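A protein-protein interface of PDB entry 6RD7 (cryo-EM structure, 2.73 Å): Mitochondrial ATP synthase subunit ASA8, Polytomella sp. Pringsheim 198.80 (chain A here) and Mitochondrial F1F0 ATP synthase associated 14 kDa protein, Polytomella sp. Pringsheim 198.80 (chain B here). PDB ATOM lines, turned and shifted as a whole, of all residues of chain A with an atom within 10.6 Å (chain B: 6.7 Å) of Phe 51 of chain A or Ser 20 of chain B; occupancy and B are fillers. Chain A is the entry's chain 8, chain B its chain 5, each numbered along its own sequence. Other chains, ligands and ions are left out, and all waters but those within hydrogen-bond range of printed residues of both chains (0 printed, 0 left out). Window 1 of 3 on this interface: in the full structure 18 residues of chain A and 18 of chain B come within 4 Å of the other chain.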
ATOM      1  N   PHE A  32     -22.494 -15.141 -36.155  1.00  0.00           N
ATOM      2  CA  PHE A  32     -23.017 -15.149 -34.798  1.00  0.00           C
ATOM      3  C   PHE A  32     -23.354 -13.744 -34.323  1.00  0.00           C
ATOM      4  O   PHE A  32     -24.222 -13.583 -33.462  1.00  0.00           O
ATOM      5  CB  PHE A  32     -22.029 -15.799 -33.831  1.00  0.00           C
ATOM      6  CG  PHE A  32     -22.559 -15.925 -32.430  1.00  0.00           C
ATOM      7  CD1 PHE A  32     -23.491 -16.896 -32.119  1.00  0.00           C
ATOM      8  CD2 PHE A  32     -22.151 -15.051 -31.436  1.00  0.00           C
ATOM      9  CE1 PHE A  32     -23.994 -17.005 -30.843  1.00  0.00           C
ATOM     10  CE2 PHE A  32     -22.657 -15.156 -30.159  1.00  0.00           C
ATOM     11  CZ  PHE A  32     -23.578 -16.136 -29.864  1.00  0.00           C
ATOM     12  N   TYR A  35     -26.922 -12.943 -35.437  1.00  0.00           N
ATOM     13  CA  TYR A  35     -27.873 -13.643 -34.584  1.00  0.00           C
ATOM     14  C   TYR A  35     -27.929 -13.031 -33.194  1.00  0.00           C
ATOM     15  O   TYR A  35     -29.000 -12.963 -32.582  1.00  0.00           O
ATOM     16  CB  TYR A  35     -27.503 -15.119 -34.499  1.00  0.00           C
ATOM     17  CG  TYR A  35     -28.276 -15.858 -33.447  1.00  0.00           C
ATOM     18  CD1 TYR A  35     -29.650 -15.991 -33.545  1.00  0.00           C
ATOM     19  CD2 TYR A  35     -27.638 -16.411 -32.346  1.00  0.00           C
ATOM     20  CE1 TYR A  35     -30.365 -16.651 -32.590  1.00  0.00           C
ATOM     21  CE2 TYR A  35     -28.349 -17.079 -31.381  1.00  0.00           C
ATOM     22  CZ  TYR A  35     -29.713 -17.197 -31.511  1.00  0.00           C
ATOM     23  OH  TYR A  35     -30.436 -17.862 -30.556  1.00  0.00           O
ATOM     24  N   LEU A  40     -30.836 -12.934 -30.664  1.00  0.00           N
ATOM     25  CA  LEU A  40     -30.503 -13.530 -29.372  1.00  0.00           C
ATOM     26  C   LEU A  40     -30.733 -12.555 -28.226  1.00  0.00           C
ATOM     27  O   LEU A  40     -31.435 -12.885 -27.267  1.00  0.00           O
ATOM     28  CB  LEU A  40     -29.066 -14.033 -29.362  1.00  0.00           C
ATOM     29  CG  LEU A  40     -28.585 -14.590 -28.026  1.00  0.00           C
ATOM     30  CD1 LEU A  40     -29.326 -15.864 -27.688  1.00  0.00           C
ATOM     31  CD2 LEU A  40     -27.094 -14.835 -28.062  1.00  0.00           C
ATOM     32  N   HIS A  44     -34.290 -13.215 -26.749  1.00  0.00           N
ATOM     33  CA  HIS A  44     -33.927 -14.237 -25.780  1.00  0.00           C
ATOM     34  C   HIS A  44     -33.163 -13.661 -24.596  1.00  0.00           C
ATOM     35  O   HIS A  44     -32.527 -14.409 -23.844  1.00  0.00           O
ATOM     36  CB  HIS A  44     -33.103 -15.340 -26.440  1.00  0.00           C
ATOM     37  CG  HIS A  44     -33.744 -15.936 -27.651  1.00  0.00           C
ATOM     38  ND1 HIS A  44     -35.060 -16.337 -27.677  1.00  0.00           N
ATOM     39  CD2 HIS A  44     -33.247 -16.205 -28.878  1.00  0.00           C
ATOM     40  CE1 HIS A  44     -35.347 -16.826 -28.867  1.00  0.00           C
ATOM     41  NE2 HIS A  44     -34.264 -16.756 -29.617  1.00  0.00           N
ATOM     42  N   TRP A  45     -33.211 -12.340 -24.401  1.00  0.00           N
ATOM     43  CA  TRP A  45     -32.539 -11.794 -23.233  1.00  0.00           C
ATOM     44  C   TRP A  45     -33.244 -12.138 -21.931  1.00  0.00           C
ATOM     45  O   TRP A  45     -32.598 -12.111 -20.884  1.00  0.00           O
ATOM     46  CB  TRP A  45     -32.369 -10.280 -23.377  1.00  0.00           C
ATOM     47  CG  TRP A  45     -33.600  -9.464 -23.167  1.00  0.00           C
ATOM     48  CD1 TRP A  45     -34.482  -9.058 -24.117  1.00  0.00           C
ATOM     49  CD2 TRP A  45     -34.064  -8.919 -21.930  1.00  0.00           C
ATOM     50  NE1 TRP A  45     -35.477  -8.310 -23.548  1.00  0.00           N
ATOM     51  CE2 TRP A  45     -35.244  -8.212 -22.204  1.00  0.00           C
ATOM     52  CE3 TRP A  45     -33.602  -8.976 -20.614  1.00  0.00           C
ATOM     53  CZ2 TRP A  45     -35.963  -7.559 -21.214  1.00  0.00           C
ATOM     54  CZ3 TRP A  45     -34.319  -8.333 -19.635  1.00  0.00           C
ATOM     55  CH2 TRP A  45     -35.487  -7.634 -19.938  1.00  0.00           C
ATOM     56  N   TYR A  46     -34.525 -12.511 -21.980  1.00  0.00           N
ATOM     57  CA  TYR A  46     -35.204 -13.029 -20.798  1.00  0.00           C
ATOM     58  C   TYR A  46     -34.596 -14.353 -20.350  1.00  0.00           C
ATOM     59  O   TYR A  46     -34.319 -14.543 -19.161  1.00  0.00           O
ATOM     60  CB  TYR A  46     -36.695 -13.196 -21.078  1.00  0.00           C
ATOM     61  CG  TYR A  46     -37.357 -12.032 -21.775  1.00  0.00           C
ATOM     62  CD1 TYR A  46     -37.852 -10.958 -21.052  1.00  0.00           C
ATOM     63  CD2 TYR A  46     -37.517 -12.022 -23.153  1.00  0.00           C
ATOM     64  CE1 TYR A  46     -38.470  -9.902 -21.682  1.00  0.00           C
ATOM     65  CE2 TYR A  46     -38.131 -10.969 -23.791  1.00  0.00           C
ATOM     66  CZ  TYR A  46     -38.605  -9.912 -23.050  1.00  0.00           C
ATOM     67  OH  TYR A  46     -39.221  -8.857 -23.681  1.00  0.00           O
ATOM     68  N   LEU A  47     -34.369 -15.276 -21.295  1.00  0.00           N
ATOM     69  CA  LEU A  47     -33.697 -16.536 -20.976  1.00  0.00           C
ATOM     70  C   LEU A  47     -32.274 -16.306 -20.509  1.00  0.00           C
ATOM     71  O   LEU A  47     -31.798 -16.985 -19.592  1.00  0.00           O
ATOM     72  CB  LEU A  47     -33.645 -17.467 -22.178  1.00  0.00           C
ATOM     73  CG  LEU A  47     -34.781 -18.224 -22.821  1.00  0.00           C
ATOM     74  CD1 LEU A  47     -34.106 -19.046 -23.889  1.00  0.00           C
ATOM     75  CD2 LEU A  47     -35.476 -19.105 -21.825  1.00  0.00           C
ATOM     76  N   LEU A  48     -31.561 -15.397 -21.176  1.00  0.00           N
ATOM     77  CA  LEU A  48     -30.179 -15.117 -20.802  1.00  0.00           C
ATOM     78  C   LEU A  48     -30.089 -14.533 -19.398  1.00  0.00           C
ATOM     79  O   LEU A  48     -29.219 -14.933 -18.614  1.00  0.00           O
ATOM     80  CB  LEU A  48     -29.550 -14.176 -21.829  1.00  0.00           C
ATOM     81  CG  LEU A  48     -28.693 -14.785 -22.942  1.00  0.00           C
ATOM     82  CD1 LEU A  48     -29.447 -15.822 -23.754  1.00  0.00           C
ATOM     83  CD2 LEU A  48     -28.184 -13.682 -23.849  1.00  0.00           C
ATOM     84  N   GLY A  49     -31.022 -13.649 -19.042  1.00  0.00           N
ATOM     85  CA  GLY A  49     -31.076 -13.143 -17.685  1.00  0.00           C
ATOM     86  C   GLY A  49     -31.509 -14.189 -16.676  1.00  0.00           C
ATOM     87  O   GLY A  49     -31.081 -14.153 -15.524  1.00  0.00           O
ATOM     88  N   GLY A  50     -32.348 -15.139 -17.093  1.00  0.00           N
ATOM     89  CA  GLY A  50     -32.736 -16.211 -16.188  1.00  0.00           C
ATOM     90  C   GLY A  50     -31.596 -17.162 -15.878  1.00  0.00           C
ATOM     91  O   GLY A  50     -31.405 -17.568 -14.725  1.00  0.00           O
ATOM     92  N   PHE A  51     -30.817 -17.520 -16.903  1.00  0.00           N
ATOM     93  CA  PHE A  51     -29.611 -18.319 -16.694  1.00  0.00           C
ATOM     94  C   PHE A  51     -28.591 -17.564 -15.852  1.00  0.00           C
ATOM     95  O   PHE A  51     -27.927 -18.156 -14.992  1.00  0.00           O
ATOM     96  CB  PHE A  51     -29.001 -18.709 -18.038  1.00  0.00           C
ATOM     97  CG  PHE A  51     -29.794 -19.733 -18.789  1.00  0.00           C
ATOM     98  CD1 PHE A  51     -30.294 -20.843 -18.143  1.00  0.00           C
ATOM     99  CD2 PHE A  51     -30.028 -19.592 -20.145  1.00  0.00           C
ATOM    100  CE1 PHE A  51     -31.027 -21.786 -18.824  1.00  0.00           C
ATOM    101  CE2 PHE A  51     -30.757 -20.534 -20.833  1.00  0.00           C
ATOM    102  CZ  PHE A  51     -31.258 -21.630 -20.169  1.00  0.00           C
ATOM    103  N   THR A  52     -28.472 -16.249 -16.076  1.00  0.00           N
ATOM    104  CA  THR A  52     -27.588 -15.411 -15.271  1.00  0.00           C
ATOM    105  C   THR A  52     -28.026 -15.380 -13.811  1.00  0.00           C
ATOM    106  O   THR A  52     -27.191 -15.485 -12.901  1.00  0.00           O
ATOM    107  CB  THR A  52     -27.562 -14.002 -15.868  1.00  0.00           C
ATOM    108  OG1 THR A  52     -26.929 -14.044 -17.151  1.00  0.00           O
ATOM    109  CG2 THR A  52     -26.807 -13.030 -14.982  1.00  0.00           C
ATOM    110  N   PHE A  53     -29.339 -15.286 -13.573  1.00  0.00           N
ATOM    111  CA  PHE A  53     -29.870 -15.286 -12.215  1.00  0.00           C
ATOM    112  C   PHE A  53     -29.611 -16.609 -11.518  1.00  0.00           C
ATOM    113  O   PHE A  53     -29.272 -16.632 -10.332  1.00  0.00           O
ATOM    114  CB  PHE A  53     -31.370 -14.992 -12.228  1.00  0.00           C
ATOM    115  CG  PHE A  53     -32.020 -15.096 -10.873  1.00  0.00           C
ATOM    116  CD1 PHE A  53     -31.890 -14.073  -9.955  1.00  0.00           C
ATOM    117  CD2 PHE A  53     -32.762 -16.215 -10.519  1.00  0.00           C
ATOM    118  CE1 PHE A  53     -32.482 -14.164  -8.713  1.00  0.00           C
ATOM    119  CE2 PHE A  53     -33.350 -16.310  -9.282  1.00  0.00           C
ATOM    120  CZ  PHE A  53     -33.213 -15.284  -8.380  1.00  0.00           C
ATOM    121  N   THR A  54     -29.771 -17.720 -12.233  1.00  0.00           N
ATOM    122  CA  THR A  54     -29.560 -19.017 -11.602  1.00  0.00           C
ATOM    123  C   THR A  54     -28.090 -19.260 -11.300  1.00  0.00           C
ATOM    124  O   THR A  54     -27.755 -19.811 -10.246  1.00  0.00           O
ATOM    125  CB  THR A  54     -30.111 -20.126 -12.479  1.00  0.00           C
ATOM    126  OG1 THR A  54     -31.397 -19.737 -12.957  1.00  0.00           O
ATOM    127  CG2 THR A  54     -30.253 -21.389 -11.679  1.00  0.00           C
ATOM    128  N   ILE A  55     -27.196 -18.827 -12.192  1.00  0.00           N
ATOM    129  CA  ILE A  55     -25.764 -18.984 -11.943  1.00  0.00           C
ATOM    130  C   ILE A  55     -25.326 -18.112 -10.766  1.00  0.00           C
ATOM    131  O   ILE A  55     -24.565 -18.558  -9.895  1.00  0.00           O
ATOM    132  CB  ILE A  55     -24.976 -18.684 -13.232  1.00  0.00           C
ATOM    133  CG1 ILE A  55     -25.194 -19.810 -14.240  1.00  0.00           C
ATOM    134  CG2 ILE A  55     -23.497 -18.542 -12.962  1.00  0.00           C
ATOM    135  CD1 ILE A  55     -24.871 -19.432 -15.661  1.00  0.00           C
ATOM    136  N   THR A  56     -25.872 -16.896 -10.671  1.00  0.00           N
ATOM    137  CA  THR A  56     -25.567 -16.012  -9.547  1.00  0.00           C
ATOM    138  C   THR A  56     -26.100 -16.571  -8.228  1.00  0.00           C
ATOM    139  O   THR A  56     -25.383 -16.598  -7.216  1.00  0.00           O
ATOM    140  CB  THR A  56     -26.146 -14.626  -9.826  1.00  0.00           C
ATOM    141  OG1 THR A  56     -25.505 -14.070 -10.978  1.00  0.00           O
ATOM    142  CG2 THR A  56     -25.935 -13.698  -8.650  1.00  0.00           C
ATOM    143  N   LEU A  57     -27.344 -17.058  -8.233  1.00  0.00           N
ATOM    144  CA  LEU A  57     -27.954 -17.594  -7.020  1.00  0.00           C
ATOM    145  C   LEU A  57     -27.258 -18.868  -6.563  1.00  0.00           C
ATOM    146  O   LEU A  57     -27.078 -19.090  -5.360  1.00  0.00           O
ATOM    147  CB  LEU A  57     -29.440 -17.846  -7.264  1.00  0.00           C
ATOM    148  CG  LEU A  57     -30.212 -18.706  -6.269  1.00  0.00           C
ATOM    149  CD1 LEU A  57     -30.529 -17.907  -5.022  1.00  0.00           C
ATOM    150  CD2 LEU A  57     -31.479 -19.243  -6.900  1.00  0.00           C
ATOM    151  N   TYR A  58     -26.808 -19.694  -7.504  1.00  0.00           N
ATOM    152  CA  TYR A  58     -26.155 -20.936  -7.116  1.00  0.00           C
ATOM    153  C   TYR A  58     -24.725 -20.677  -6.670  1.00  0.00           C
ATOM    154  O   TYR A  58     -24.184 -21.420  -5.846  1.00  0.00           O
ATOM    155  CB  TYR A  58     -26.209 -21.942  -8.263  1.00  0.00           C
ATOM    156  CG  TYR A  58     -27.494 -22.739  -8.311  1.00  0.00           C
ATOM    157  CD1 TYR A  58     -28.727 -22.111  -8.205  1.00  0.00           C
ATOM    158  CD2 TYR A  58     -27.475 -24.113  -8.461  1.00  0.00           C
ATOM    159  CE1 TYR A  58     -29.890 -22.818  -8.245  1.00  0.00           C
ATOM    160  CE2 TYR A  58     -28.643 -24.834  -8.505  1.00  0.00           C
ATOM    161  CZ  TYR A  58     -29.844 -24.174  -8.395  1.00  0.00           C
ATOM    162  OH  TYR A  58     -31.018 -24.864  -8.433  1.00  0.00           O
ATOM    163  N   GLY A  59     -24.112 -19.598  -7.162  1.00  0.00           N
ATOM    164  CA  GLY A  59     -22.852 -19.159  -6.586  1.00  0.00           C
ATOM    165  C   GLY A  59     -23.009 -18.663  -5.162  1.00  0.00           C
ATOM    166  O   GLY A  59     -22.150 -18.910  -4.310  1.00  0.00           O
ATOM    167  N   ALA B  12     -25.212 -25.795 -12.459  1.00  0.00           N
ATOM    168  CA  ALA B  12     -26.199 -24.882 -13.025  1.00  0.00           C
ATOM    169  C   ALA B  12     -25.661 -24.184 -14.266  1.00  0.00           C
ATOM    170  O   ALA B  12     -26.411 -23.928 -15.214  1.00  0.00           O
ATOM    171  CB  ALA B  12     -26.629 -23.855 -11.984  1.00  0.00           C
ATOM    172  N   ALA B  13     -24.360 -23.895 -14.296  1.00  0.00           N
ATOM    173  CA  ALA B  13     -23.764 -23.301 -15.484  1.00  0.00           C
ATOM    174  C   ALA B  13     -23.641 -24.321 -16.603  1.00  0.00           C
ATOM    175  O   ALA B  13     -23.702 -23.959 -17.779  1.00  0.00           O
ATOM    176  CB  ALA B  13     -22.403 -22.704 -15.146  1.00  0.00           C
ATOM    177  N   ALA B  15     -25.953 -26.654 -17.062  1.00  0.00           N
ATOM    178  CA  ALA B  15     -27.322 -26.626 -17.575  1.00  0.00           C
ATOM    179  C   ALA B  15     -27.574 -25.405 -18.449  1.00  0.00           C
ATOM    180  O   ALA B  15     -28.199 -25.515 -19.509  1.00  0.00           O
ATOM    181  CB  ALA B  15     -28.317 -26.666 -16.419  1.00  0.00           C
ATOM    182  N   ALA B  16     -27.063 -24.242 -18.035  1.00  0.00           N
ATOM    183  CA  ALA B  16     -27.228 -23.024 -18.820  1.00  0.00           C
ATOM    184  C   ALA B  16     -26.477 -23.086 -20.141  1.00  0.00           C
ATOM    185  O   ALA B  16     -26.999 -22.633 -21.161  1.00  0.00           O
ATOM    186  CB  ALA B  16     -26.767 -21.813 -18.014  1.00  0.00           C
ATOM    187  N   VAL B  17     -25.275 -23.664 -20.151  1.00  0.00           N
ATOM    188  CA  VAL B  17     -24.487 -23.759 -21.376  1.00  0.00           C
ATOM    189  C   VAL B  17     -25.125 -24.744 -22.348  1.00  0.00           C
ATOM    190  O   VAL B  17     -25.222 -24.471 -23.552  1.00  0.00           O
ATOM    191  CB  VAL B  17     -23.030 -24.128 -21.036  1.00  0.00           C
ATOM    192  CG1 VAL B  17     -22.299 -24.734 -22.219  1.00  0.00           C
ATOM    193  CG2 VAL B  17     -22.295 -22.891 -20.573  1.00  0.00           C
ATOM    194  N   VAL B  18     -25.626 -25.874 -21.834  1.00  0.00           N
ATOM    195  CA  VAL B  18     -26.273 -26.863 -22.695  1.00  0.00           C
ATOM    196  C   VAL B  18     -27.573 -26.311 -23.273  1.00  0.00           C
ATOM    197  O   VAL B  18     -27.832 -26.436 -24.476  1.00  0.00           O
ATOM    198  CB  VAL B  18     -26.496 -28.176 -21.920  1.00  0.00           C
ATOM    199  CG1 VAL B  18     -27.424 -29.096 -22.665  1.00  0.00           C
ATOM    200  CG2 VAL B  18     -25.179 -28.879 -21.701  1.00  0.00           C
ATOM    201  N   ALA B  19     -28.374 -25.629 -22.451  1.00  0.00           N
ATOM    202  CA  ALA B  19     -29.636 -25.093 -22.947  1.00  0.00           C
ATOM    203  C   ALA B  19     -29.422 -23.889 -23.857  1.00  0.00           C
ATOM    204  O   ALA B  19     -30.194 -23.677 -24.795  1.00  0.00           O
ATOM    205  CB  ALA B  19     -30.547 -24.738 -21.779  1.00  0.00           C
ATOM    206  N   SER B  20     -28.358 -23.114 -23.633  1.00  0.00           N
ATOM    207  CA  SER B  20     -28.054 -22.004 -24.527  1.00  0.00           C
ATOM    208  C   SER B  20     -27.529 -22.500 -25.863  1.00  0.00           C
ATOM    209  O   SER B  20     -27.815 -21.900 -26.905  1.00  0.00           O
ATOM    210  CB  SER B  20     -27.043 -21.067 -23.875  1.00  0.00           C
ATOM    211  OG  SER B  20     -27.590 -20.467 -22.719  1.00  0.00           O
ATOM    212  N   TRP B  21     -26.771 -23.599 -25.860  1.00  0.00           N
ATOM    213  CA  TRP B  21     -26.357 -24.193 -27.122  1.00  0.00           C
ATOM    214  C   TRP B  21     -27.542 -24.776 -27.873  1.00  0.00           C
ATOM    215  O   TRP B  21     -27.604 -24.672 -29.100  1.00  0.00           O
ATOM    216  CB  TRP B  21     -25.303 -25.275 -26.906  1.00  0.00           C
ATOM    217  CG  TRP B  21     -24.770 -25.782 -28.208  1.00  0.00           C
ATOM    218  CD1 TRP B  21     -23.734 -25.266 -28.914  1.00  0.00           C
ATOM    219  CD2 TRP B  21     -25.269 -26.883 -28.980  1.00  0.00           C
ATOM    220  NE1 TRP B  21     -23.545 -25.977 -30.067  1.00  0.00           N
ATOM    221  CE2 TRP B  21     -24.478 -26.975 -30.132  1.00  0.00           C
ATOM    222  CE3 TRP B  21     -26.310 -27.799 -28.804  1.00  0.00           C
ATOM    223  CZ2 TRP B  21     -24.687 -27.945 -31.103  1.00  0.00           C
ATOM    224  CZ3 TRP B  21     -26.517 -28.756 -29.766  1.00  0.00           C
ATOM    225  CH2 TRP B  21     -25.709 -28.825 -30.901  1.00  0.00           C
ATOM    226  N   VAL B  22     -28.476 -25.412 -27.162  1.00  0.00           N
ATOM    227  CA  VAL B  22     -29.660 -25.959 -27.819  1.00  0.00           C
ATOM    228  C   VAL B  22     -30.526 -24.832 -28.371  1.00  0.00           C
ATOM    229  O   VAL B  22     -31.071 -24.937 -29.474  1.00  0.00           O
ATOM    230  CB  VAL B  22     -30.429 -26.880 -26.851  1.00  0.00           C
ATOM    231  CG1 VAL B  22     -31.789 -27.265 -27.395  1.00  0.00           C
ATOM    232  CG2 VAL B  22     -29.637 -28.138 -26.609  1.00  0.00           C
ATOM    233  N   LEU B  23     -30.585 -23.704 -27.660  1.00  0.00           N
ATOM    234  CA  LEU B  23     -31.320 -22.541 -28.145  1.00  0.00           C
ATOM    235  C   LEU B  23     -30.676 -21.943 -29.389  1.00  0.00           C
ATOM    236  O   LEU B  23     -31.375 -21.619 -30.355  1.00  0.00           O
ATOM    237  CB  LEU B  23     -31.409 -21.488 -27.045  1.00  0.00           C
ATOM    238  CG  LEU B  23     -31.960 -20.128 -27.453  1.00  0.00           C
ATOM    239  CD1 LEU B  23     -33.470 -20.157 -27.478  1.00  0.00           C
ATOM    240  CD2 LEU B  23     -31.442 -19.053 -26.531  1.00  0.00           C
ATOM    241  N   TRP B  24     -29.347 -21.794 -29.385  1.00  0.00           N
ATOM    242  CA  TRP B  24     -28.647 -21.276 -30.556  1.00  0.00           C
ATOM    243  C   TRP B  24     -28.775 -22.220 -31.742  1.00  0.00           C
ATOM    244  O   TRP B  24     -28.974 -21.777 -32.876  1.00  0.00           O
ATOM    245  CB  TRP B  24     -27.170 -21.034 -30.237  1.00  0.00           C
ATOM    246  CG  TRP B  24     -26.332 -20.814 -31.468  1.00  0.00           C
ATOM    247  CD1 TRP B  24     -26.135 -19.640 -32.120  1.00  0.00           C
ATOM    248  CD2 TRP B  24     -25.590 -21.801 -32.194  1.00  0.00           C
ATOM    249  NE1 TRP B  24     -25.324 -19.830 -33.206  1.00  0.00           N
ATOM    250  CE2 TRP B  24     -24.981 -21.152 -33.276  1.00  0.00           C
ATOM    251  CE3 TRP B  24     -25.399 -23.175 -32.039  1.00  0.00           C
ATOM    252  CZ2 TRP B  24     -24.186 -21.823 -34.191  1.00  0.00           C
ATOM    253  CZ3 TRP B  24     -24.617 -23.837 -32.948  1.00  0.00           C
ATOM    254  CH2 TRP B  24     -24.017 -23.163 -34.009  1.00  0.00           C
ATOM    255  N   HIS B  25     -28.662 -23.524 -31.501  1.00  0.00           N
ATOM    256  CA  HIS B  25     -28.707 -24.484 -32.595  1.00  0.00           C
ATOM    257  C   HIS B  25     -30.114 -24.629 -33.140  1.00  0.00           C
ATOM    258  O   HIS B  25     -30.302 -24.915 -34.325  1.00  0.00           O
ATOM    259  CB  HIS B  25     -28.169 -25.828 -32.124  1.00  0.00           C
ATOM    260  CG  HIS B  25     -27.854 -26.769 -33.240  1.00  0.00           C
ATOM    261  ND1 HIS B  25     -28.739 -27.730 -33.668  1.00  0.00           N
ATOM    262  CD2 HIS B  25     -26.757 -26.891 -34.019  1.00  0.00           C
ATOM    263  CE1 HIS B  25     -28.201 -28.406 -34.665  1.00  0.00           C
ATOM    264  NE2 HIS B  25     -26.998 -27.916 -34.897  1.00  0.00           N
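Phe 51 of chain A touches three residues of chain B.
Of chain A, only Phe 51 comes within 4 Å of Ser 20 of chain B.
Of chain A, only Phe 51 (3.6 Å) comes within 4 Å of Ala 19 of chain B.
Printed residues of chain A within 4 Å of Ala 13 of chain B: Ile 55.
Printed residues of chain A within 4 Å of Trp 24 of chain B: Phe 32 (3.6 Å) and Tyr 35 (3.5 Å).
The nearest residue of chain B that does not touch Phe 51 of chain A is Ala 15 of chain B (4.7 Å).
The nearest printed residue of chain A that does not touch Trp 24 of chain B is Leu 40 of chain A (6.2 Å).
The backbone NH (N) of Leu 40 of chain A sits at hydrogen-bond distance from the backbone carbonyl oxygen (O) of Tyr 35 of chain A, at 2.7 Å.
The backbone NH of Trp 45 of chain A is in hydrogen-bond range of the backbone carbonyl oxygen of Leu 40 of chain A (3.4 Å).
The backbone carbonyl oxygen (O) of Ala 16 of chain B sits at hydrogen-bond distance from the side-chain hydroxyl (OG) of Ser 20 of chain B (2.7 Å).
Phe 32 of chain A touches Trp 24 of chain B (CD1 to NE1, 3.6 Å).
Trp 24 of chain B touches Tyr 35 of chain A (CD1 to CE2, 3.5 Å).
CD2 of Leu 23 of chain B touches CD1 of Leu 40 of chain A, at 3.998 Å.
Leu 23 of chain B touches Leu 47 of chain A.
CB of Ala 16 of chain B touches CD1 of Phe 51 of chain A (3.7 Å).
Phe 51 of chain A touches Ala 19 of chain B.
Ser 20 of chain B touches Phe 51 of chain A.
CA of Ala 13 of chain B touches CG1 of Ile 55 of chain A, at 3.97 Å.
Ala 16 of chain B touches Ile 55 of chain A.
Tyr 58 of chain A touches Ala 12 of chain B (CD2 to CB, 3.6 Å).
Of the 13 printed residues of chain B, 7 touch a printed residue of chain A.
Printed residues of chain B that touch a printed residue of chain A: Ala 12, Ala 13, Ala 16, Ala 19, Ser 20, Leu 23 and Trp 24.
Hydrophobic or aromatic side chains of chain B within 4 Å of the printed part of chain A: Ala 12, Ala 16, Ala 19, Leu 23 and Trp 24.
Along chain B the printed residues that touch a printed residue of chain A span positions 12 to 24.
Of the 19 printed residues of chain A, 7 touch a printed residue of chain B.
Hydrophobic or aromatic side chains of chain A that line the printed part of chain B: Phe 32, Tyr 35, Leu 40, Leu 47, Phe 51, Ile 55 and Tyr 58.
Among the printed residues, 11 pairs touch across the chains.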
